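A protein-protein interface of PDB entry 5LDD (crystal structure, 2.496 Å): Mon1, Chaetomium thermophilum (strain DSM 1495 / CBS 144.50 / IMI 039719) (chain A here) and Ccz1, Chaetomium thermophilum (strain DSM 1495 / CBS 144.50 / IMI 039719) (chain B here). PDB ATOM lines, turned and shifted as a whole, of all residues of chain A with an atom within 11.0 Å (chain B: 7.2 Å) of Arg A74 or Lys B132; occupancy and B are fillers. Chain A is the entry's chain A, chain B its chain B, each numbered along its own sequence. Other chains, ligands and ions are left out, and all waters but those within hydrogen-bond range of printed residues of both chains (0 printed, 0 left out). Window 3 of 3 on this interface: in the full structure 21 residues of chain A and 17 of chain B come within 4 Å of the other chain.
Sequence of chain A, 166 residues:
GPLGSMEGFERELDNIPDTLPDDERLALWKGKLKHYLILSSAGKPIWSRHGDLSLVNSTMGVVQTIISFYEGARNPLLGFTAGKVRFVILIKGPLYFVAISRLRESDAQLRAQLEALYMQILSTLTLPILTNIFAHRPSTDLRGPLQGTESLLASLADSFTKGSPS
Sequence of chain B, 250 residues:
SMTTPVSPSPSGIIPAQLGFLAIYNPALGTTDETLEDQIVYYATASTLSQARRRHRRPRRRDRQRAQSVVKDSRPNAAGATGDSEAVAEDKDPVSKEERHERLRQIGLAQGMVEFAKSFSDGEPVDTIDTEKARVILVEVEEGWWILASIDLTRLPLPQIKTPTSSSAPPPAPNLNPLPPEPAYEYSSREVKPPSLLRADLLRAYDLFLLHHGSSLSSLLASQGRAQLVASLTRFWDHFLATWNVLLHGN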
ATOM      1  N   ILE A  66     -20.587  16.841 -35.480  1.00  0.00           N
ATOM      2  CA  ILE A  66     -21.148  15.613 -34.925  1.00  0.00           C
ATOM      3  C   ILE A  66     -20.081  14.841 -34.170  1.00  0.00           C
ATOM      4  O   ILE A  66     -20.311  14.342 -33.059  1.00  0.00           O
ATOM      5  CB  ILE A  66     -21.763  14.752 -36.042  1.00  0.00           C
ATOM      6  CG1 ILE A  66     -23.027  15.403 -36.595  1.00  0.00           C
ATOM      7  CG2 ILE A  66     -22.028  13.357 -35.535  1.00  0.00           C
ATOM      8  CD1 ILE A  66     -23.610  14.659 -37.768  1.00  0.00           C
ATOM      9  N   ILE A  67     -18.901  14.714 -34.770  1.00  0.00           N
ATOM     10  CA  ILE A  67     -17.801  14.038 -34.089  1.00  0.00           C
ATOM     11  C   ILE A  67     -17.411  14.786 -32.818  1.00  0.00           C
ATOM     12  O   ILE A  67     -17.072  14.171 -31.796  1.00  0.00           O
ATOM     13  CB  ILE A  67     -16.615  13.896 -35.057  1.00  0.00           C
ATOM     14  CG1 ILE A  67     -17.009  12.969 -36.214  1.00  0.00           C
ATOM     15  CG2 ILE A  67     -15.352  13.443 -34.329  1.00  0.00           C
ATOM     16  CD1 ILE A  67     -15.949  12.871 -37.302  1.00  0.00           C
ATOM     17  N   SER A  68     -17.498  16.120 -32.846  1.00  0.00           N
ATOM     18  CA  SER A  68     -17.066  16.925 -31.703  1.00  0.00           C
ATOM     19  C   SER A  68     -17.996  16.779 -30.509  1.00  0.00           C
ATOM     20  O   SER A  68     -17.551  16.920 -29.362  1.00  0.00           O
ATOM     21  CB  SER A  68     -16.972  18.395 -32.096  1.00  0.00           C
ATOM     22  OG  SER A  68     -16.012  18.589 -33.123  1.00  0.00           O
ATOM     23  N   PHE A  69     -19.288  16.537 -30.748  1.00  0.00           N
ATOM     24  CA  PHE A  69     -20.198  16.299 -29.633  1.00  0.00           C
ATOM     25  C   PHE A  69     -19.738  15.098 -28.820  1.00  0.00           C
ATOM     26  O   PHE A  69     -19.720  15.134 -27.583  1.00  0.00           O
ATOM     27  CB  PHE A  69     -21.629  16.088 -30.143  1.00  0.00           C
ATOM     28  CG  PHE A  69     -22.456  17.352 -30.218  1.00  0.00           C
ATOM     29  CD1 PHE A  69     -22.174  18.331 -31.165  1.00  0.00           C
ATOM     30  CD2 PHE A  69     -23.535  17.545 -29.362  1.00  0.00           C
ATOM     31  CE1 PHE A  69     -22.935  19.499 -31.251  1.00  0.00           C
ATOM     32  CE2 PHE A  69     -24.308  18.708 -29.440  1.00  0.00           C
ATOM     33  CZ  PHE A  69     -24.005  19.691 -30.395  1.00  0.00           C
ATOM     34  N   TYR A  70     -19.352  14.023 -29.504  1.00  0.00           N
ATOM     35  CA  TYR A  70     -18.918  12.826 -28.804  1.00  0.00           C
ATOM     36  C   TYR A  70     -17.520  12.983 -28.220  1.00  0.00           C
ATOM     37  O   TYR A  70     -17.242  12.434 -27.147  1.00  0.00           O
ATOM     38  CB  TYR A  70     -19.000  11.633 -29.745  1.00  0.00           C
ATOM     39  CG  TYR A  70     -20.422  11.256 -30.069  1.00  0.00           C
ATOM     40  CD1 TYR A  70     -21.182  10.500 -29.174  1.00  0.00           C
ATOM     41  CD2 TYR A  70     -21.007  11.641 -31.265  1.00  0.00           C
ATOM     42  CE1 TYR A  70     -22.486  10.141 -29.465  1.00  0.00           C
ATOM     43  CE2 TYR A  70     -22.307  11.288 -31.565  1.00  0.00           C
ATOM     44  CZ  TYR A  70     -23.041  10.538 -30.662  1.00  0.00           C
ATOM     45  OH  TYR A  70     -24.334  10.191 -30.967  1.00  0.00           O
ATOM     46  N   GLU A  71     -16.647  13.758 -28.870  1.00  0.00           N
ATOM     47  CA  GLU A  71     -15.372  14.095 -28.244  1.00  0.00           C
ATOM     48  C   GLU A  71     -15.611  14.877 -26.965  1.00  0.00           C
ATOM     49  O   GLU A  71     -15.034  14.568 -25.914  1.00  0.00           O
ATOM     50  CB  GLU A  71     -14.491  14.900 -29.201  1.00  0.00           C
ATOM     51  CG  GLU A  71     -13.973  14.109 -30.391  1.00  0.00           C
ATOM     52  CD  GLU A  71     -13.085  12.958 -29.973  1.00  0.00           C
ATOM     53  OE1 GLU A  71     -12.019  13.204 -29.351  1.00  0.00           O
ATOM     54  OE2 GLU A  71     -13.458  11.803 -30.267  1.00  0.00           O
ATOM     55  N   GLY A  72     -16.502  15.871 -27.026  1.00  0.00           N
ATOM     56  CA  GLY A  72     -16.807  16.646 -25.838  1.00  0.00           C
ATOM     57  C   GLY A  72     -17.394  15.806 -24.723  1.00  0.00           C
ATOM     58  O   GLY A  72     -17.164  16.085 -23.546  1.00  0.00           O
ATOM     59  N   ALA A  73     -18.150  14.770 -25.070  1.00  0.00           N
ATOM     60  CA  ALA A  73     -18.697  13.870 -24.068  1.00  0.00           C
ATOM     61  C   ALA A  73     -17.684  12.845 -23.588  1.00  0.00           C
ATOM     62  O   ALA A  73     -18.042  11.994 -22.766  1.00  0.00           O
ATOM     63  CB  ALA A  73     -19.926  13.154 -24.623  1.00  0.00           C
ATOM     64  N   ARG A  74     -16.440  12.910 -24.070  1.00  0.00           N
ATOM     65  CA  ARG A  74     -15.408  11.923 -23.735  1.00  0.00           C
ATOM     66  C   ARG A  74     -15.875  10.512 -24.100  1.00  0.00           C
ATOM     67  O   ARG A  74     -15.599   9.542 -23.390  1.00  0.00           O
ATOM     68  CB  ARG A  74     -15.017  12.016 -22.257  1.00  0.00           C
ATOM     69  CG  ARG A  74     -13.693  11.356 -21.898  1.00  0.00           C
ATOM     70  CD  ARG A  74     -12.502  12.195 -22.324  1.00  0.00           C
ATOM     71  NE  ARG A  74     -12.446  13.458 -21.597  1.00  0.00           N
ATOM     72  CZ  ARG A  74     -11.402  14.278 -21.612  1.00  0.00           C
ATOM     73  NH1 ARG A  74     -11.439  15.409 -20.923  1.00  0.00           N
ATOM     74  NH2 ARG A  74     -10.319  13.966 -22.313  1.00  0.00           N
ATOM     75  N   ASN A  75     -16.617  10.403 -25.205  1.00  0.00           N
ATOM     76  CA  ASN A  75     -17.177   9.134 -25.670  1.00  0.00           C
ATOM     77  C   ASN A  75     -17.113   9.083 -27.190  1.00  0.00           C
ATOM     78  O   ASN A  75     -18.115   9.320 -27.878  1.00  0.00           O
ATOM     79  CB  ASN A  75     -18.617   8.967 -25.182  1.00  0.00           C
ATOM     80  CG  ASN A  75     -19.266   7.689 -25.687  1.00  0.00           C
ATOM     81  OD1 ASN A  75     -18.582   6.749 -26.105  1.00  0.00           O
ATOM     82  ND2 ASN A  75     -20.597   7.655 -25.668  1.00  0.00           N
ATOM     83  N   PRO A  76     -15.953   8.730 -27.750  1.00  0.00           N
ATOM     84  CA  PRO A  76     -15.742   8.873 -29.202  1.00  0.00           C
ATOM     85  C   PRO A  76     -16.757   8.125 -30.057  1.00  0.00           C
ATOM     86  O   PRO A  76     -17.235   7.044 -29.708  1.00  0.00           O
ATOM     87  CB  PRO A  76     -14.333   8.307 -29.409  1.00  0.00           C
ATOM     88  CG  PRO A  76     -13.653   8.511 -28.097  1.00  0.00           C
ATOM     89  CD  PRO A  76     -14.731   8.289 -27.057  1.00  0.00           C
ATOM     90  N   LEU A  77     -17.052   8.716 -31.215  1.00  0.00           N
ATOM     91  CA  LEU A  77     -18.020   8.175 -32.159  1.00  0.00           C
ATOM     92  C   LEU A  77     -17.329   7.211 -33.118  1.00  0.00           C
ATOM     93  O   LEU A  77     -16.404   7.602 -33.838  1.00  0.00           O
ATOM     94  CB  LEU A  77     -18.679   9.311 -32.934  1.00  0.00           C
ATOM     95  CG  LEU A  77     -19.570   8.903 -34.100  1.00  0.00           C
ATOM     96  CD1 LEU A  77     -20.764   8.118 -33.585  1.00  0.00           C
ATOM     97  CD2 LEU A  77     -20.039  10.133 -34.854  1.00  0.00           C
ATOM     98  N   LEU A  78     -17.806   5.965 -33.155  1.00  0.00           N
ATOM     99  CA  LEU A  78     -17.250   4.935 -34.026  1.00  0.00           C
ATOM    100  C   LEU A  78     -17.988   4.803 -35.349  1.00  0.00           C
ATOM    101  O   LEU A  78     -17.353   4.527 -36.374  1.00  0.00           O
ATOM    102  CB  LEU A  78     -17.257   3.578 -33.316  1.00  0.00           C
ATOM    103  CG  LEU A  78     -16.482   3.546 -31.993  1.00  0.00           C
ATOM    104  CD1 LEU A  78     -16.576   2.182 -31.318  1.00  0.00           C
ATOM    105  CD2 LEU A  78     -15.026   3.937 -32.237  1.00  0.00           C
ATOM    106  N   GLY A  79     -19.299   5.007 -35.362  1.00  0.00           N
ATOM    107  CA  GLY A  79     -20.044   4.910 -36.600  1.00  0.00           C
ATOM    108  C   GLY A  79     -21.524   4.848 -36.319  1.00  0.00           C
ATOM    109  O   GLY A  79     -21.963   4.762 -35.168  1.00  0.00           O
ATOM    110  N   ILE A  91     -10.489   8.310 -36.284  1.00  0.00           N
ATOM    111  CA  ILE A  91      -9.805   9.513 -35.827  1.00  0.00           C
ATOM    112  C   ILE A  91      -8.338   9.169 -35.588  1.00  0.00           C
ATOM    113  O   ILE A  91      -8.022   8.228 -34.848  1.00  0.00           O
ATOM    114  CB  ILE A  91     -10.445  10.091 -34.559  1.00  0.00           C
ATOM    115  CG1 ILE A  91     -11.872  10.542 -34.840  1.00  0.00           C
ATOM    116  CG2 ILE A  91      -9.625  11.260 -34.051  1.00  0.00           C
ATOM    117  CD1 ILE A  91     -12.608  10.993 -33.599  1.00  0.00           C
ATOM    118  N   ASP B 129     -22.955   3.758 -32.797  1.00  0.00           N
ATOM    119  CA  ASP B 129     -21.967   2.988 -32.053  1.00  0.00           C
ATOM    120  C   ASP B 129     -20.889   3.932 -31.537  1.00  0.00           C
ATOM    121  O   ASP B 129     -20.187   4.569 -32.330  1.00  0.00           O
ATOM    122  CB  ASP B 129     -21.375   1.888 -32.929  1.00  0.00           C
ATOM    123  CG  ASP B 129     -22.425   0.877 -33.373  1.00  0.00           C
ATOM    124  OD1 ASP B 129     -22.834   0.043 -32.531  1.00  0.00           O
ATOM    125  OD2 ASP B 129     -22.845   0.914 -34.556  1.00  0.00           O
ATOM    126  N   THR B 130     -20.776   4.043 -30.215  1.00  0.00           N
ATOM    127  CA  THR B 130     -19.739   4.856 -29.594  1.00  0.00           C
ATOM    128  C   THR B 130     -18.833   3.965 -28.764  1.00  0.00           C
ATOM    129  O   THR B 130     -19.104   2.780 -28.565  1.00  0.00           O
ATOM    130  CB  THR B 130     -20.327   5.964 -28.711  1.00  0.00           C
ATOM    131  OG1 THR B 130     -20.940   5.382 -27.554  1.00  0.00           O
ATOM    132  CG2 THR B 130     -21.372   6.736 -29.478  1.00  0.00           C
ATOM    133  N   GLU B 131     -17.743   4.557 -28.274  1.00  0.00           N
ATOM    134  CA  GLU B 131     -16.773   3.785 -27.504  1.00  0.00           C
ATOM    135  C   GLU B 131     -17.392   3.238 -26.222  1.00  0.00           C
ATOM    136  O   GLU B 131     -17.090   2.118 -25.810  1.00  0.00           O
ATOM    137  CB  GLU B 131     -15.552   4.644 -27.183  1.00  0.00           C
ATOM    138  CG  GLU B 131     -14.549   3.958 -26.257  1.00  0.00           C
ATOM    139  CD  GLU B 131     -13.368   4.844 -25.884  1.00  0.00           C
ATOM    140  OE1 GLU B 131     -13.564   5.827 -25.136  1.00  0.00           O
ATOM    141  OE2 GLU B 131     -12.241   4.553 -26.338  1.00  0.00           O
ATOM    142  N   LYS B 132     -18.281   4.002 -25.594  1.00  0.00           N
ATOM    143  CA  LYS B 132     -18.808   3.655 -24.283  1.00  0.00           C
ATOM    144  C   LYS B 132     -20.293   3.331 -24.286  1.00  0.00           C
ATOM    145  O   LYS B 132     -20.804   2.862 -23.264  1.00  0.00           O
ATOM    146  CB  LYS B 132     -18.537   4.800 -23.299  1.00  0.00           C
ATOM    147  CG  LYS B 132     -17.049   5.083 -23.129  1.00  0.00           C
ATOM    148  CD  LYS B 132     -16.799   6.301 -22.264  1.00  0.00           C
ATOM    149  CE  LYS B 132     -15.310   6.597 -22.173  1.00  0.00           C
ATOM    150  NZ  LYS B 132     -15.043   7.802 -21.341  1.00  0.00           N
ATOM    151  N   ALA B 133     -21.005   3.572 -25.382  1.00  0.00           N
ATOM    152  CA  ALA B 133     -22.442   3.357 -25.385  1.00  0.00           C
ATOM    153  C   ALA B 133     -22.902   2.833 -26.734  1.00  0.00           C
ATOM    154  O   ALA B 133     -22.310   3.130 -27.775  1.00  0.00           O
ATOM    155  CB  ALA B 133     -23.217   4.635 -25.043  1.00  0.00           C
ATOM    156  N   ARG B 134     -23.971   2.048 -26.688  1.00  0.00           N
ATOM    157  CA  ARG B 134     -24.711   1.594 -27.855  1.00  0.00           C
ATOM    158  C   ARG B 134     -26.029   2.348 -27.880  1.00  0.00           C
ATOM    159  O   ARG B 134     -26.829   2.224 -26.950  1.00  0.00           O
ATOM    160  CB  ARG B 134     -24.950   0.088 -27.791  1.00  0.00           C
ATOM    161  CG  ARG B 134     -26.127  -0.386 -28.638  1.00  0.00           C
ATOM    162  CD  ARG B 134     -26.086  -1.887 -28.778  1.00  0.00           C
ATOM    163  NE  ARG B 134     -24.846  -2.267 -29.434  1.00  0.00           N
ATOM    164  CZ  ARG B 134     -24.392  -3.508 -29.516  1.00  0.00           C
ATOM    165  NH1 ARG B 134     -25.083  -4.502 -28.978  1.00  0.00           N
ATOM    166  NH2 ARG B 134     -23.243  -3.750 -30.131  1.00  0.00           N
ATOM    167  N   SER B 149     -29.908   5.211 -24.935  1.00  0.00           N
ATOM    168  CA  SER B 149     -28.466   5.025 -24.859  1.00  0.00           C
ATOM    169  C   SER B 149     -28.167   4.002 -23.767  1.00  0.00           C
ATOM    170  O   SER B 149     -28.509   4.216 -22.599  1.00  0.00           O
ATOM    171  CB  SER B 149     -27.783   6.364 -24.578  1.00  0.00           C
ATOM    172  OG  SER B 149     -26.373   6.242 -24.518  1.00  0.00           O
ATOM    173  N   ILE B 150     -27.537   2.891 -24.143  1.00  0.00           N
ATOM    174  CA  ILE B 150     -27.204   1.818 -23.211  1.00  0.00           C
ATOM    175  C   ILE B 150     -25.711   1.881 -22.935  1.00  0.00           C
ATOM    176  O   ILE B 150     -24.898   1.678 -23.848  1.00  0.00           O
ATOM    177  CB  ILE B 150     -27.598   0.433 -23.756  1.00  0.00           C
ATOM    178  CG1 ILE B 150     -29.110   0.211 -23.659  1.00  0.00           C
ATOM    179  CG2 ILE B 150     -26.862  -0.671 -22.985  1.00  0.00           C
ATOM    180  CD1 ILE B 150     -29.927   0.911 -24.725  1.00  0.00           C
ATOM    181  N   ASP B 151     -25.350   2.156 -21.682  1.00  0.00           N
ATOM    182  CA  ASP B 151     -23.948   2.144 -21.289  1.00  0.00           C
ATOM    183  C   ASP B 151     -23.389   0.733 -21.375  1.00  0.00           C
ATOM    184  O   ASP B 151     -24.027  -0.225 -20.941  1.00  0.00           O
ATOM    185  CB  ASP B 151     -23.782   2.689 -19.874  1.00  0.00           C
ATOM    186  CG  ASP B 151     -23.951   4.190 -19.802  1.00  0.00           C
ATOM    187  OD1 ASP B 151     -23.583   4.873 -20.781  1.00  0.00           O
ATOM    188  OD2 ASP B 151     -24.432   4.689 -18.761  1.00  0.00           O
ATOM    189  N   LEU B 152     -22.191   0.606 -21.938  1.00  0.00           N
ATOM    190  CA  LEU B 152     -21.585  -0.706 -22.098  1.00  0.00           C
ATOM    191  C   LEU B 152     -20.975  -1.185 -20.780  1.00  0.00           C
ATOM    192  O   LEU B 152     -20.898  -0.456 -19.789  1.00  0.00           O
ATOM    193  CB  LEU B 152     -20.526  -0.673 -23.199  1.00  0.00           C
ATOM    194  CG  LEU B 152     -21.006  -0.335 -24.612  1.00  0.00           C
ATOM    195  CD1 LEU B 152     -19.851  -0.408 -25.593  1.00  0.00           C
ATOM    196  CD2 LEU B 152     -22.117  -1.276 -25.034  1.00  0.00           C
ATOM    197  N   THR B 153     -20.546  -2.441 -20.773  1.00  0.00           N
ATOM    198  CA  THR B 153     -19.938  -2.998 -19.577  1.00  0.00           C
ATOM    199  C   THR B 153     -18.567  -2.374 -19.348  1.00  0.00           C
ATOM    200  O   THR B 153     -17.703  -2.404 -20.230  1.00  0.00           O
ATOM    201  CB  THR B 153     -19.825  -4.515 -19.695  1.00  0.00           C
ATOM    202  OG1 THR B 153     -21.137  -5.076 -19.839  1.00  0.00           O
ATOM    203  CG2 THR B 153     -19.181  -5.087 -18.441  1.00  0.00           C
ATOM    204  N   ARG B 154     -18.373  -1.811 -18.160  1.00  0.00           N
ATOM    205  CA  ARG B 154     -17.115  -1.196 -17.757  1.00  0.00           C
ATOM    206  C   ARG B 154     -16.302  -2.215 -16.969  1.00  0.00           C
ATOM    207  O   ARG B 154     -16.740  -2.676 -15.909  1.00  0.00           O
ATOM    208  CB  ARG B 154     -17.357   0.045 -16.899  1.00  0.00           C
ATOM    209  CG  ARG B 154     -18.358   1.038 -17.441  1.00  0.00           C
ATOM    210  CD  ARG B 154     -18.661   2.089 -16.382  1.00  0.00           C
ATOM    211  NE  ARG B 154     -17.559   3.029 -16.199  1.00  0.00           N
ATOM    212  CZ  ARG B 154     -17.622   4.119 -15.438  1.00  0.00           C
ATOM    213  NH1 ARG B 154     -18.740   4.411 -14.786  1.00  0.00           N
ATOM    214  NH2 ARG B 154     -16.568   4.916 -15.326  1.00  0.00           N
ATOM    215  N   TYR B 184     -11.173   2.558 -17.741  1.00  0.00           N
ATOM    216  CA  TYR B 184     -11.586   1.168 -17.904  1.00  0.00           C
ATOM    217  C   TYR B 184     -11.629   0.766 -19.377  1.00  0.00           C
ATOM    218  O   TYR B 184     -11.370   1.576 -20.270  1.00  0.00           O
ATOM    219  CB  TYR B 184     -12.968   0.936 -17.277  1.00  0.00           C
ATOM    220  CG  TYR B 184     -13.127   1.448 -15.862  1.00  0.00           C
ATOM    221  CD1 TYR B 184     -12.058   1.445 -14.971  1.00  0.00           C
ATOM    222  CD2 TYR B 184     -14.350   1.939 -15.417  1.00  0.00           C
ATOM    223  CE1 TYR B 184     -12.205   1.916 -13.676  1.00  0.00           C
ATOM    224  CE2 TYR B 184     -14.508   2.411 -14.126  1.00  0.00           C
ATOM    225  CZ  TYR B 184     -13.433   2.398 -13.260  1.00  0.00           C
ATOM    226  OH  TYR B 184     -13.583   2.865 -11.973  1.00  0.00           O
ATOM    227  N   TYR B 186     -14.221  -1.104 -22.288  1.00  0.00           N
ATOM    228  CA  TYR B 186     -15.654  -1.181 -22.533  1.00  0.00           C
ATOM    229  C   TYR B 186     -15.967  -2.336 -23.471  1.00  0.00           C
ATOM    230  O   TYR B 186     -15.250  -2.570 -24.446  1.00  0.00           O
ATOM    231  CB  TYR B 186     -16.167   0.141 -23.105  1.00  0.00           C
ATOM    232  CG  TYR B 186     -15.882   1.308 -22.195  1.00  0.00           C
ATOM    233  CD1 TYR B 186     -16.829   1.745 -21.286  1.00  0.00           C
ATOM    234  CD2 TYR B 186     -14.655   1.961 -22.230  1.00  0.00           C
ATOM    235  CE1 TYR B 186     -16.574   2.807 -20.443  1.00  0.00           C
ATOM    236  CE2 TYR B 186     -14.386   3.020 -21.387  1.00  0.00           C
ATOM    237  CZ  TYR B 186     -15.351   3.443 -20.495  1.00  0.00           C
ATOM    238  OH  TYR B 186     -15.102   4.503 -19.651  1.00  0.00           O
ATOM    239  N   SER B 187     -17.032  -3.070 -23.159  1.00  0.00           N
ATOM    240  CA  SER B 187     -17.386  -4.268 -23.903  1.00  0.00           C
ATOM    241  C   SER B 187     -18.874  -4.281 -24.202  1.00  0.00           C
ATOM    242  O   SER B 187     -19.689  -3.795 -23.412  1.00  0.00           O
ATOM    243  CB  SER B 187     -17.001  -5.544 -23.126  1.00  0.00           C
ATOM    244  OG  SER B 187     -17.528  -6.700 -23.755  1.00  0.00           O
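Tyr A70 touches Thr B130. CA of Thr B130 touches O of Pro A76, 3.3 Å away. CD1 of Leu A77 touches O of Asp B129, 3.8 Å away. CD1 of Leu A78 touches O of Thr B130, at 3.8 Å.
Of the 15 printed residues of chain B, 4 touch a printed residue of chain A. Printed residues of chain A that touch a printed residue of chain B: Tyr A70, Arg A74, Asn A75, Pro A76, Leu A77, Leu A78 and Gly A79. Along chain A the printed residues that touch a printed residue of chain B span positions 70 to 79. Among the printed residues, 11 pairs touch across the chains. Among the printed residues, no Asp or Glu carboxylate lies within 4 Å of a Lys or Arg side-chain nitrogen of the other chain.
N of Asn A75 sits at hydrogen-bond distance from O of Tyr A70, 2.9 Å away. The backbone carbonyl oxygen (O) of Ala B133 is in hydrogen-bond range of the side-chain hydroxyl (OG1) of Thr B130 (2.6 Å). The backbone carbonyl oxygen of Lys B132 lies within hydrogen-bond range of the backbone NH of Leu B152, at 3.0 Å.
Arg A74 touches one residue of chain B. Of chain A, only Arg A74 (2.7 Å) and Asn A75 (2.8 Å) come within 4 Å of Lys B132. Of the printed residues of chain A, Thr B130 touches Tyr A70, Asn A75, Pro A76 and Leu A78. No residue of chain A comes within 4 Å of Ala B133. No residue of chain A comes within 4 Å of Asp B151. No residue of chain A comes within 4 Å of Leu B152. Printed residues of chain A within 4 Å of Asp B129: Leu A77 (3.8 Å), Leu A78 (2.9 Å) and Gly A79 (2.8 Å). Of the printed residues of chain B, Asn A75 touches Thr B130 (3.0 Å), Glu B131 (3.2 Å) and Lys B132 (2.8 Å). Ser A68 touches none of the printed residues of chain B.
OG1 of Thr B130 is in hydrogen-bond range of ND2 of Asn A75 (3.0 Å). O of Pro A76 lies within hydrogen-bond range of N of Glu B131, at 2.9 Å. The backbone carbonyl oxygen (O) of Arg A74 lies within hydrogen-bond range of the side-chain amino group (NZ) of Lys B132 (2.7 Å). The backbone NH (N) of Lys B132 sits at hydrogen-bond distance from the side-chain amide oxygen (OD1) of Asn A75, at 2.8 Å. The side-chain amide oxygen (OD1) of Asn A75 sits at hydrogen-bond distance from the backbone NH (N) of Glu B131 (3.2 Å). The backbone NH (N) of Asp B129 is in hydrogen-bond range of the backbone carbonyl oxygen (O) of Gly A79 (2.8 Å). The backbone NH of Leu A78 lies within hydrogen-bond range of the backbone carbonyl oxygen of Asp B129, 2.9 Å away.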
